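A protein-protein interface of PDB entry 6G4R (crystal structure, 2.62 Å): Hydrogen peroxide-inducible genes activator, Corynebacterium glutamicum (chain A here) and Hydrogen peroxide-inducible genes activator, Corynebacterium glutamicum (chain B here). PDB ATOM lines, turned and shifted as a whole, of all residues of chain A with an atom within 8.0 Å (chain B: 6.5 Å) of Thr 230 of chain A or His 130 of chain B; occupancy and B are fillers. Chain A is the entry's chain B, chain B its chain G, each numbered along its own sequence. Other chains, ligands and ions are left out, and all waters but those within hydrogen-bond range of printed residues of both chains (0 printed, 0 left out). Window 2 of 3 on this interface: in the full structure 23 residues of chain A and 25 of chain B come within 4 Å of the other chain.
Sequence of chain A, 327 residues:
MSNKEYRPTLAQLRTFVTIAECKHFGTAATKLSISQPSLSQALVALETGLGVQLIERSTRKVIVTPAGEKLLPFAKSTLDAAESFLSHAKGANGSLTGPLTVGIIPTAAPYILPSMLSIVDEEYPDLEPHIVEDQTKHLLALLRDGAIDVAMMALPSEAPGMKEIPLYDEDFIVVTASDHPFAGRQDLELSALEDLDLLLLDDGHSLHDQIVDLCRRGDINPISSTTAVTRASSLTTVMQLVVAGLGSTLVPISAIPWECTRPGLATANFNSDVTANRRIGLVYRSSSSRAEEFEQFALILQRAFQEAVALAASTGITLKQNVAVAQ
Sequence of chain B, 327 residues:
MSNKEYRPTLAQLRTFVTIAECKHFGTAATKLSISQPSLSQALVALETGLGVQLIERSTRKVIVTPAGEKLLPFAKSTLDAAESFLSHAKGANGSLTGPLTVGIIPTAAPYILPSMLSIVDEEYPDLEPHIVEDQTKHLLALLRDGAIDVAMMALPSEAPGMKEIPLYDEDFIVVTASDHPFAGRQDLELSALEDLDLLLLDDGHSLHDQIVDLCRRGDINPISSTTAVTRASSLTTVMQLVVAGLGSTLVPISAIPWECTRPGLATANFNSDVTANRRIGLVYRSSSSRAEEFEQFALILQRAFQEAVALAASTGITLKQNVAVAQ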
ATOM      1  N   LEU A 198      16.337   9.771  16.729  1.00  0.00           N
ATOM      2  CA  LEU A 198      15.413   8.657  16.902  1.00  0.00           C
ATOM      3  C   LEU A 198      14.436   8.570  15.736  1.00  0.00           C
ATOM      4  O   LEU A 198      13.914   9.582  15.259  1.00  0.00           O
ATOM      5  CB  LEU A 198      14.649   8.805  18.216  1.00  0.00           C
ATOM      6  CG  LEU A 198      15.485   8.776  19.496  1.00  0.00           C
ATOM      7  CD1 LEU A 198      14.651   9.203  20.695  1.00  0.00           C
ATOM      8  CD2 LEU A 198      16.076   7.393  19.717  1.00  0.00           C
ATOM      9  N   LEU A 199      14.191   7.343  15.279  1.00  0.00           N
ATOM     10  CA  LEU A 199      13.153   7.040  14.295  1.00  0.00           C
ATOM     11  C   LEU A 199      12.011   6.339  15.020  1.00  0.00           C
ATOM     12  O   LEU A 199      12.182   5.232  15.541  1.00  0.00           O
ATOM     13  CB  LEU A 199      13.679   6.180  13.145  1.00  0.00           C
ATOM     14  CG  LEU A 199      14.728   6.683  12.144  1.00  0.00           C
ATOM     15  CD1 LEU A 199      15.167   8.125  12.392  1.00  0.00           C
ATOM     16  CD2 LEU A 199      15.923   5.741  12.105  1.00  0.00           C
ATOM     17  N   LEU A 200      10.859   6.994  15.058  1.00  0.00           N
ATOM     18  CA  LEU A 200       9.711   6.564  15.838  1.00  0.00           C
ATOM     19  C   LEU A 200       8.582   6.096  14.929  1.00  0.00           C
ATOM     20  O   LEU A 200       8.468   6.514  13.773  1.00  0.00           O
ATOM     21  CB  LEU A 200       9.203   7.686  16.749  1.00  0.00           C
ATOM     22  CG  LEU A 200      10.215   8.330  17.699  1.00  0.00           C
ATOM     23  CD1 LEU A 200       9.634   9.587  18.330  1.00  0.00           C
ATOM     24  CD2 LEU A 200      10.642   7.338  18.771  1.00  0.00           C
ATOM     25  N   LEU A 201       7.751   5.217  15.478  1.00  0.00           N
ATOM     26  CA  LEU A 201       6.508   4.822  14.842  1.00  0.00           C
ATOM     27  C   LEU A 201       5.512   5.977  14.946  1.00  0.00           C
ATOM     28  O   LEU A 201       5.690   6.913  15.733  1.00  0.00           O
ATOM     29  CB  LEU A 201       5.950   3.563  15.505  1.00  0.00           C
ATOM     30  CG  LEU A 201       6.738   2.268  15.273  1.00  0.00           C
ATOM     31  CD1 LEU A 201       6.393   1.212  16.320  1.00  0.00           C
ATOM     32  CD2 LEU A 201       6.503   1.732  13.875  1.00  0.00           C
ATOM     33  N   ASP A 202       4.478   5.932  14.110  1.00  0.00           N
ATOM     34  CA  ASP A 202       3.534   7.041  13.992  1.00  0.00           C
ATOM     35  C   ASP A 202       2.759   7.226  15.301  1.00  0.00           C
ATOM     36  O   ASP A 202       3.012   6.564  16.311  1.00  0.00           O
ATOM     37  CB  ASP A 202       2.580   6.804  12.823  1.00  0.00           C
ATOM     38  CG  ASP A 202       1.761   5.524  12.983  1.00  0.00           C
ATOM     39  OD1 ASP A 202       1.953   4.809  13.985  1.00  0.00           O
ATOM     40  OD2 ASP A 202       0.910   5.235  12.113  1.00  0.00           O
ATOM     41  N   SER A 225      12.436  15.139  16.672  1.00  0.00           N
ATOM     42  CA  SER A 225      12.280  13.739  16.296  1.00  0.00           C
ATOM     43  C   SER A 225      10.836  13.337  16.037  1.00  0.00           C
ATOM     44  O   SER A 225      10.591  12.452  15.211  1.00  0.00           O
ATOM     45  CB  SER A 225      12.861  12.830  17.385  1.00  0.00           C
ATOM     46  OG  SER A 225      12.186  13.013  18.616  1.00  0.00           O
ATOM     47  N   THR A 226       9.875  13.961  16.719  1.00  0.00           N
ATOM     48  CA  THR A 226       8.479  13.572  16.556  1.00  0.00           C
ATOM     49  C   THR A 226       7.846  14.265  15.356  1.00  0.00           C
ATOM     50  O   THR A 226       7.147  13.629  14.561  1.00  0.00           O
ATOM     51  CB  THR A 226       7.700  13.889  17.830  1.00  0.00           C
ATOM     52  OG1 THR A 226       7.613  15.310  17.996  1.00  0.00           O
ATOM     53  CG2 THR A 226       8.410  13.292  19.027  1.00  0.00           C
ATOM     54  N   THR A 227       8.079  15.569  15.212  1.00  0.00           N
ATOM     55  CA  THR A 227       7.589  16.321  14.065  1.00  0.00           C
ATOM     56  C   THR A 227       8.465  16.155  12.833  1.00  0.00           C
ATOM     57  O   THR A 227       8.408  16.998  11.929  1.00  0.00           O
ATOM     58  CB  THR A 227       7.465  17.807  14.418  1.00  0.00           C
ATOM     59  OG1 THR A 227       8.701  18.274  14.974  1.00  0.00           O
ATOM     60  CG2 THR A 227       6.341  18.027  15.419  1.00  0.00           C
ATOM     61  N   ALA A 228       9.271  15.096  12.770  1.00  0.00           N
ATOM     62  CA  ALA A 228      10.123  14.878  11.614  1.00  0.00           C
ATOM     63  C   ALA A 228       9.280  14.433  10.421  1.00  0.00           C
ATOM     64  O   ALA A 228       8.067  14.222  10.518  1.00  0.00           O
ATOM     65  CB  ALA A 228      11.206  13.851  11.940  1.00  0.00           C
ATOM     66  N   VAL A 229       9.937  14.279   9.275  1.00  0.00           N
ATOM     67  CA  VAL A 229       9.245  13.887   8.052  1.00  0.00           C
ATOM     68  C   VAL A 229       9.207  12.371   7.900  1.00  0.00           C
ATOM     69  O   VAL A 229       8.152  11.789   7.628  1.00  0.00           O
ATOM     70  CB  VAL A 229       9.905  14.565   6.833  1.00  0.00           C
ATOM     71  CG1 VAL A 229       9.386  13.956   5.539  1.00  0.00           C
ATOM     72  CG2 VAL A 229       9.688  16.070   6.872  1.00  0.00           C
ATOM     73  N   THR A 230      10.356  11.714   8.070  1.00  0.00           N
ATOM     74  CA  THR A 230      10.423  10.262   7.953  1.00  0.00           C
ATOM     75  C   THR A 230       9.545   9.605   9.011  1.00  0.00           C
ATOM     76  O   THR A 230       9.587   9.972  10.189  1.00  0.00           O
ATOM     77  CB  THR A 230      11.871   9.785   8.092  1.00  0.00           C
ATOM     78  OG1 THR A 230      12.676  10.388   7.071  1.00  0.00           O
ATOM     79  CG2 THR A 230      11.950   8.272   7.960  1.00  0.00           C
ATOM     80  N   ARG A 231       8.744   8.629   8.586  1.00  0.00           N
ATOM     81  CA  ARG A 231       7.745   8.031   9.469  1.00  0.00           C
ATOM     82  C   ARG A 231       7.413   6.638   8.960  1.00  0.00           C
ATOM     83  O   ARG A 231       7.031   6.481   7.796  1.00  0.00           O
ATOM     84  CB  ARG A 231       6.495   8.915   9.517  1.00  0.00           C
ATOM     85  CG  ARG A 231       5.481   8.559  10.589  1.00  0.00           C
ATOM     86  CD  ARG A 231       4.407   9.639  10.675  1.00  0.00           C
ATOM     87  NE  ARG A 231       3.921  10.017   9.351  1.00  0.00           N
ATOM     88  CZ  ARG A 231       2.991   9.348   8.678  1.00  0.00           C
ATOM     89  NH1 ARG A 231       2.442   8.263   9.207  1.00  0.00           N
ATOM     90  NH2 ARG A 231       2.611   9.760   7.476  1.00  0.00           N
ATOM     91  N   ALA A 232       7.554   5.634   9.823  1.00  0.00           N
ATOM     92  CA  ALA A 232       7.266   4.250   9.477  1.00  0.00           C
ATOM     93  C   ALA A 232       6.149   3.705  10.358  1.00  0.00           C
ATOM     94  O   ALA A 232       5.868   4.228  11.439  1.00  0.00           O
ATOM     95  CB  ALA A 232       8.515   3.369   9.614  1.00  0.00           C
ATOM     96  N   THR A 237      10.435  -1.968   9.074  1.00  0.00           N
ATOM     97  CA  THR A 237      10.806  -0.844   8.219  1.00  0.00           C
ATOM     98  C   THR A 237      11.765   0.097   8.937  1.00  0.00           C
ATOM     99  O   THR A 237      12.713   0.609   8.331  1.00  0.00           O
ATOM    100  CB  THR A 237       9.555  -0.096   7.760  1.00  0.00           C
ATOM    101  OG1 THR A 237       8.695  -0.994   7.047  1.00  0.00           O
ATOM    102  CG2 THR A 237       9.926   1.066   6.851  1.00  0.00           C
ATOM    103  N   VAL A 238      11.529   0.338  10.230  1.00  0.00           N
ATOM    104  CA  VAL A 238      12.445   1.156  11.020  1.00  0.00           C
ATOM    105  C   VAL A 238      13.837   0.536  11.032  1.00  0.00           C
ATOM    106  O   VAL A 238      14.850   1.243  10.957  1.00  0.00           O
ATOM    107  CB  VAL A 238      11.893   1.344  12.446  1.00  0.00           C
ATOM    108  CG1 VAL A 238      12.930   2.001  13.342  1.00  0.00           C
ATOM    109  CG2 VAL A 238      10.618   2.169  12.413  1.00  0.00           C
ATOM    110  N   LEU A 241      15.918   1.389   8.042  1.00  0.00           N
ATOM    111  CA  LEU A 241      16.439   2.750   8.101  1.00  0.00           C
ATOM    112  C   LEU A 241      17.644   2.847   9.026  1.00  0.00           C
ATOM    113  O   LEU A 241      18.567   3.626   8.762  1.00  0.00           O
ATOM    114  CB  LEU A 241      15.341   3.713   8.551  1.00  0.00           C
ATOM    115  CG  LEU A 241      14.071   3.722   7.701  1.00  0.00           C
ATOM    116  CD1 LEU A 241      13.065   4.717   8.254  1.00  0.00           C
ATOM    117  CD2 LEU A 241      14.402   4.040   6.250  1.00  0.00           C
ATOM    118  N   LEU A 246      20.282   6.152   9.023  1.00  0.00           N
ATOM    119  CA  LEU A 246      19.410   7.316   9.084  1.00  0.00           C
ATOM    120  C   LEU A 246      18.857   7.558  10.484  1.00  0.00           C
ATOM    121  O   LEU A 246      17.850   8.258  10.632  1.00  0.00           O
ATOM    122  CB  LEU A 246      18.265   7.173   8.081  1.00  0.00           C
ATOM    123  CG  LEU A 246      18.647   7.026   6.605  1.00  0.00           C
ATOM    124  CD1 LEU A 246      17.434   7.241   5.712  1.00  0.00           C
ATOM    125  CD2 LEU A 246      19.768   7.983   6.230  1.00  0.00           C
ATOM    126  N   PRO B  99      16.176  17.459  -0.404  1.00  0.00           N
ATOM    127  CA  PRO B  99      15.220  16.496   0.146  1.00  0.00           C
ATOM    128  C   PRO B  99      14.306  15.929  -0.925  1.00  0.00           C
ATOM    129  O   PRO B  99      14.005  16.575  -1.933  1.00  0.00           O
ATOM    130  CB  PRO B  99      14.427  17.324   1.167  1.00  0.00           C
ATOM    131  CG  PRO B  99      15.291  18.504   1.461  1.00  0.00           C
ATOM    132  CD  PRO B  99      15.986  18.800   0.168  1.00  0.00           C
ATOM    133  N   LEU B 100      13.867  14.696  -0.693  1.00  0.00           N
ATOM    134  CA  LEU B 100      12.879  14.052  -1.553  1.00  0.00           C
ATOM    135  C   LEU B 100      12.060  13.117  -0.676  1.00  0.00           C
ATOM    136  O   LEU B 100      12.555  12.065  -0.259  1.00  0.00           O
ATOM    137  CB  LEU B 100      13.545  13.296  -2.699  1.00  0.00           C
ATOM    138  CG  LEU B 100      12.602  12.556  -3.651  1.00  0.00           C
ATOM    139  CD1 LEU B 100      11.664  13.532  -4.343  1.00  0.00           C
ATOM    140  CD2 LEU B 100      13.391  11.750  -4.672  1.00  0.00           C
ATOM    141  N   THR B 101      10.819  13.502  -0.396  1.00  0.00           N
ATOM    142  CA  THR B 101       9.938  12.721   0.462  1.00  0.00           C
ATOM    143  C   THR B 101       9.151  11.737  -0.395  1.00  0.00           C
ATOM    144  O   THR B 101       8.388  12.144  -1.278  1.00  0.00           O
ATOM    145  CB  THR B 101       8.994  13.633   1.244  1.00  0.00           C
ATOM    146  OG1 THR B 101       9.760  14.610   1.960  1.00  0.00           O
ATOM    147  CG2 THR B 101       8.170  12.823   2.230  1.00  0.00           C
ATOM    148  N   VAL B 102       9.337  10.447  -0.132  1.00  0.00           N
ATOM    149  CA  VAL B 102       8.729   9.379  -0.916  1.00  0.00           C
ATOM    150  C   VAL B 102       7.863   8.530   0.003  1.00  0.00           C
ATOM    151  O   VAL B 102       8.304   8.127   1.086  1.00  0.00           O
ATOM    152  CB  VAL B 102       9.795   8.522  -1.623  1.00  0.00           C
ATOM    153  CG1 VAL B 102      10.997   8.319  -0.718  1.00  0.00           C
ATOM    154  CG2 VAL B 102       9.213   7.182  -2.050  1.00  0.00           C
ATOM    155  N   GLY B 103       6.629   8.271  -0.425  1.00  0.00           N
ATOM    156  CA  GLY B 103       5.720   7.405   0.303  1.00  0.00           C
ATOM    157  C   GLY B 103       5.699   6.019  -0.312  1.00  0.00           C
ATOM    158  O   GLY B 103       5.625   5.870  -1.534  1.00  0.00           O
ATOM    159  N   GLU B 128      18.667  13.674  -0.117  1.00  0.00           N
ATOM    160  CA  GLU B 128      18.276  13.563   1.287  1.00  0.00           C
ATOM    161  C   GLU B 128      16.907  12.898   1.334  1.00  0.00           C
ATOM    162  O   GLU B 128      15.870  13.581   1.337  1.00  0.00           O
ATOM    163  CB  GLU B 128      18.265  14.936   1.959  1.00  0.00           C
ATOM    164  CG  GLU B 128      17.862  14.928   3.425  1.00  0.00           C
ATOM    165  CD  GLU B 128      17.639  16.326   3.968  1.00  0.00           C
ATOM    166  OE1 GLU B 128      18.320  17.261   3.497  1.00  0.00           O
ATOM    167  OE2 GLU B 128      16.788  16.489   4.867  1.00  0.00           O
ATOM    168  N   PRO B 129      16.853  11.568   1.363  1.00  0.00           N
ATOM    169  CA  PRO B 129      15.563  10.880   1.259  1.00  0.00           C
ATOM    170  C   PRO B 129      14.827  10.821   2.588  1.00  0.00           C
ATOM    171  O   PRO B 129      15.424  10.642   3.652  1.00  0.00           O
ATOM    172  CB  PRO B 129      15.955   9.477   0.783  1.00  0.00           C
ATOM    173  CG  PRO B 129      17.329   9.269   1.330  1.00  0.00           C
ATOM    174  CD  PRO B 129      17.984  10.627   1.451  1.00  0.00           C
ATOM    175  N   HIS B 130      13.507  10.976   2.510  1.00  0.00           N
ATOM    176  CA  HIS B 130      12.618  10.834   3.653  1.00  0.00           C
ATOM    177  C   HIS B 130      11.525   9.840   3.290  1.00  0.00           C
ATOM    178  O   HIS B 130      10.879   9.980   2.247  1.00  0.00           O
ATOM    179  CB  HIS B 130      12.009  12.180   4.057  1.00  0.00           C
ATOM    180  CG  HIS B 130      13.019  13.201   4.480  1.00  0.00           C
ATOM    181  ND1 HIS B 130      13.694  13.126   5.680  1.00  0.00           N
ATOM    182  CD2 HIS B 130      13.463  14.324   3.868  1.00  0.00           C
ATOM    183  CE1 HIS B 130      14.515  14.157   5.785  1.00  0.00           C
ATOM    184  NE2 HIS B 130      14.392  14.899   4.700  1.00  0.00           N
ATOM    185  N   ILE B 131      11.322   8.842   4.146  1.00  0.00           N
ATOM    186  CA  ILE B 131      10.444   7.713   3.859  1.00  0.00           C
ATOM    187  C   ILE B 131       9.179   7.846   4.696  1.00  0.00           C
ATOM    188  O   ILE B 131       9.249   8.081   5.908  1.00  0.00           O
ATOM    189  CB  ILE B 131      11.146   6.374   4.139  1.00  0.00           C
ATOM    190  CG1 ILE B 131      12.515   6.334   3.457  1.00  0.00           C
ATOM    191  CG2 ILE B 131      10.282   5.212   3.675  1.00  0.00           C
ATOM    192  CD1 ILE B 131      12.449   6.383   1.950  1.00  0.00           C
ATOM    193  N   VAL B 132       8.026   7.683   4.050  1.00  0.00           N
ATOM    194  CA  VAL B 132       6.729   7.688   4.719  1.00  0.00           C
ATOM    195  C   VAL B 132       6.031   6.382   4.366  1.00  0.00           C
ATOM    196  O   VAL B 132       5.660   6.162   3.205  1.00  0.00           O
ATOM    197  CB  VAL B 132       5.874   8.897   4.318  1.00  0.00           C
ATOM    198  CG1 VAL B 132       4.470   8.760   4.880  1.00  0.00           C
ATOM    199  CG2 VAL B 132       6.519  10.187   4.798  1.00  0.00           C
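OG1 of Thr 230 of chain A sits at hydrogen-bond distance from ND1 of His 130 of chain B (3.2 Å).
The backbone NH (N) of Arg 231 of chain A is in hydrogen-bond range of the backbone carbonyl oxygen (O) of Ile 131 of chain B (2.8 Å).
O of Leu 100 of chain B is in hydrogen-bond range of N of His 130 of chain B (3.1 Å).
The backbone NH of Val 102 of chain B sits at hydrogen-bond distance from the backbone carbonyl oxygen of His 130 of chain B (2.9 Å).
The backbone carbonyl oxygen of Val 102 of chain B sits at hydrogen-bond distance from the backbone NH of Val 132 of chain B, 3.0 Å away.
The side-chain carboxylate (OE2) of Glu 128 of chain B sits at hydrogen-bond distance from a ring nitrogen (NE2) of His 130 of chain B (2.9 Å).
Among the printed residues, merely in contact across the chains: Val 229 of chain A with Thr 101 of chain B (3.7 Å), Val 229 of chain A with His 130 of chain B (3.5 Å), Val 229 of chain A with Val 132 of chain B (3.6 Å), Thr 230 of chain A with Ile 131 of chain B (3.2 Å) and Arg 231 of chain A with Val 132 of chain B (3.3 Å).
Thr 230 of chain A touches just these residues of chain B: His 130 and Ile 131.
His 130 of chain B touches two residues of chain A.
Of the printed residues of chain A, Thr 101 of chain B touches Val 229 (3.7 Å).
Of the printed residues of chain B, Arg 231 of chain A touches Ile 131 and Val 132.
Of the printed residues of chain A, Ile 131 of chain B touches Thr 230 (3.2 Å) and Arg 231 (2.8 Å).
Printed residues of chain A within 4 Å of Val 132 of chain B: Val 229 (3.6 Å) and Arg 231 (3.3 Å).
Gly 103 of chain B touches none of the printed residues of chain A.
The nearest residue of chain A that does not touch His 130 of chain B is Arg 231 of chain A (6.1 Å).
Of the 17 printed residues of chain A, 3 touch a printed residue of chain B.
Of the 10 printed residues of chain B, 4 touch a printed residue of chain A.
Among the printed residues, 7 pairs touch across the chains.
Among the printed residues, no Asp or Glu carboxylate lies within 4 Å of a Lys or Arg side-chain nitrogen of the other chain.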
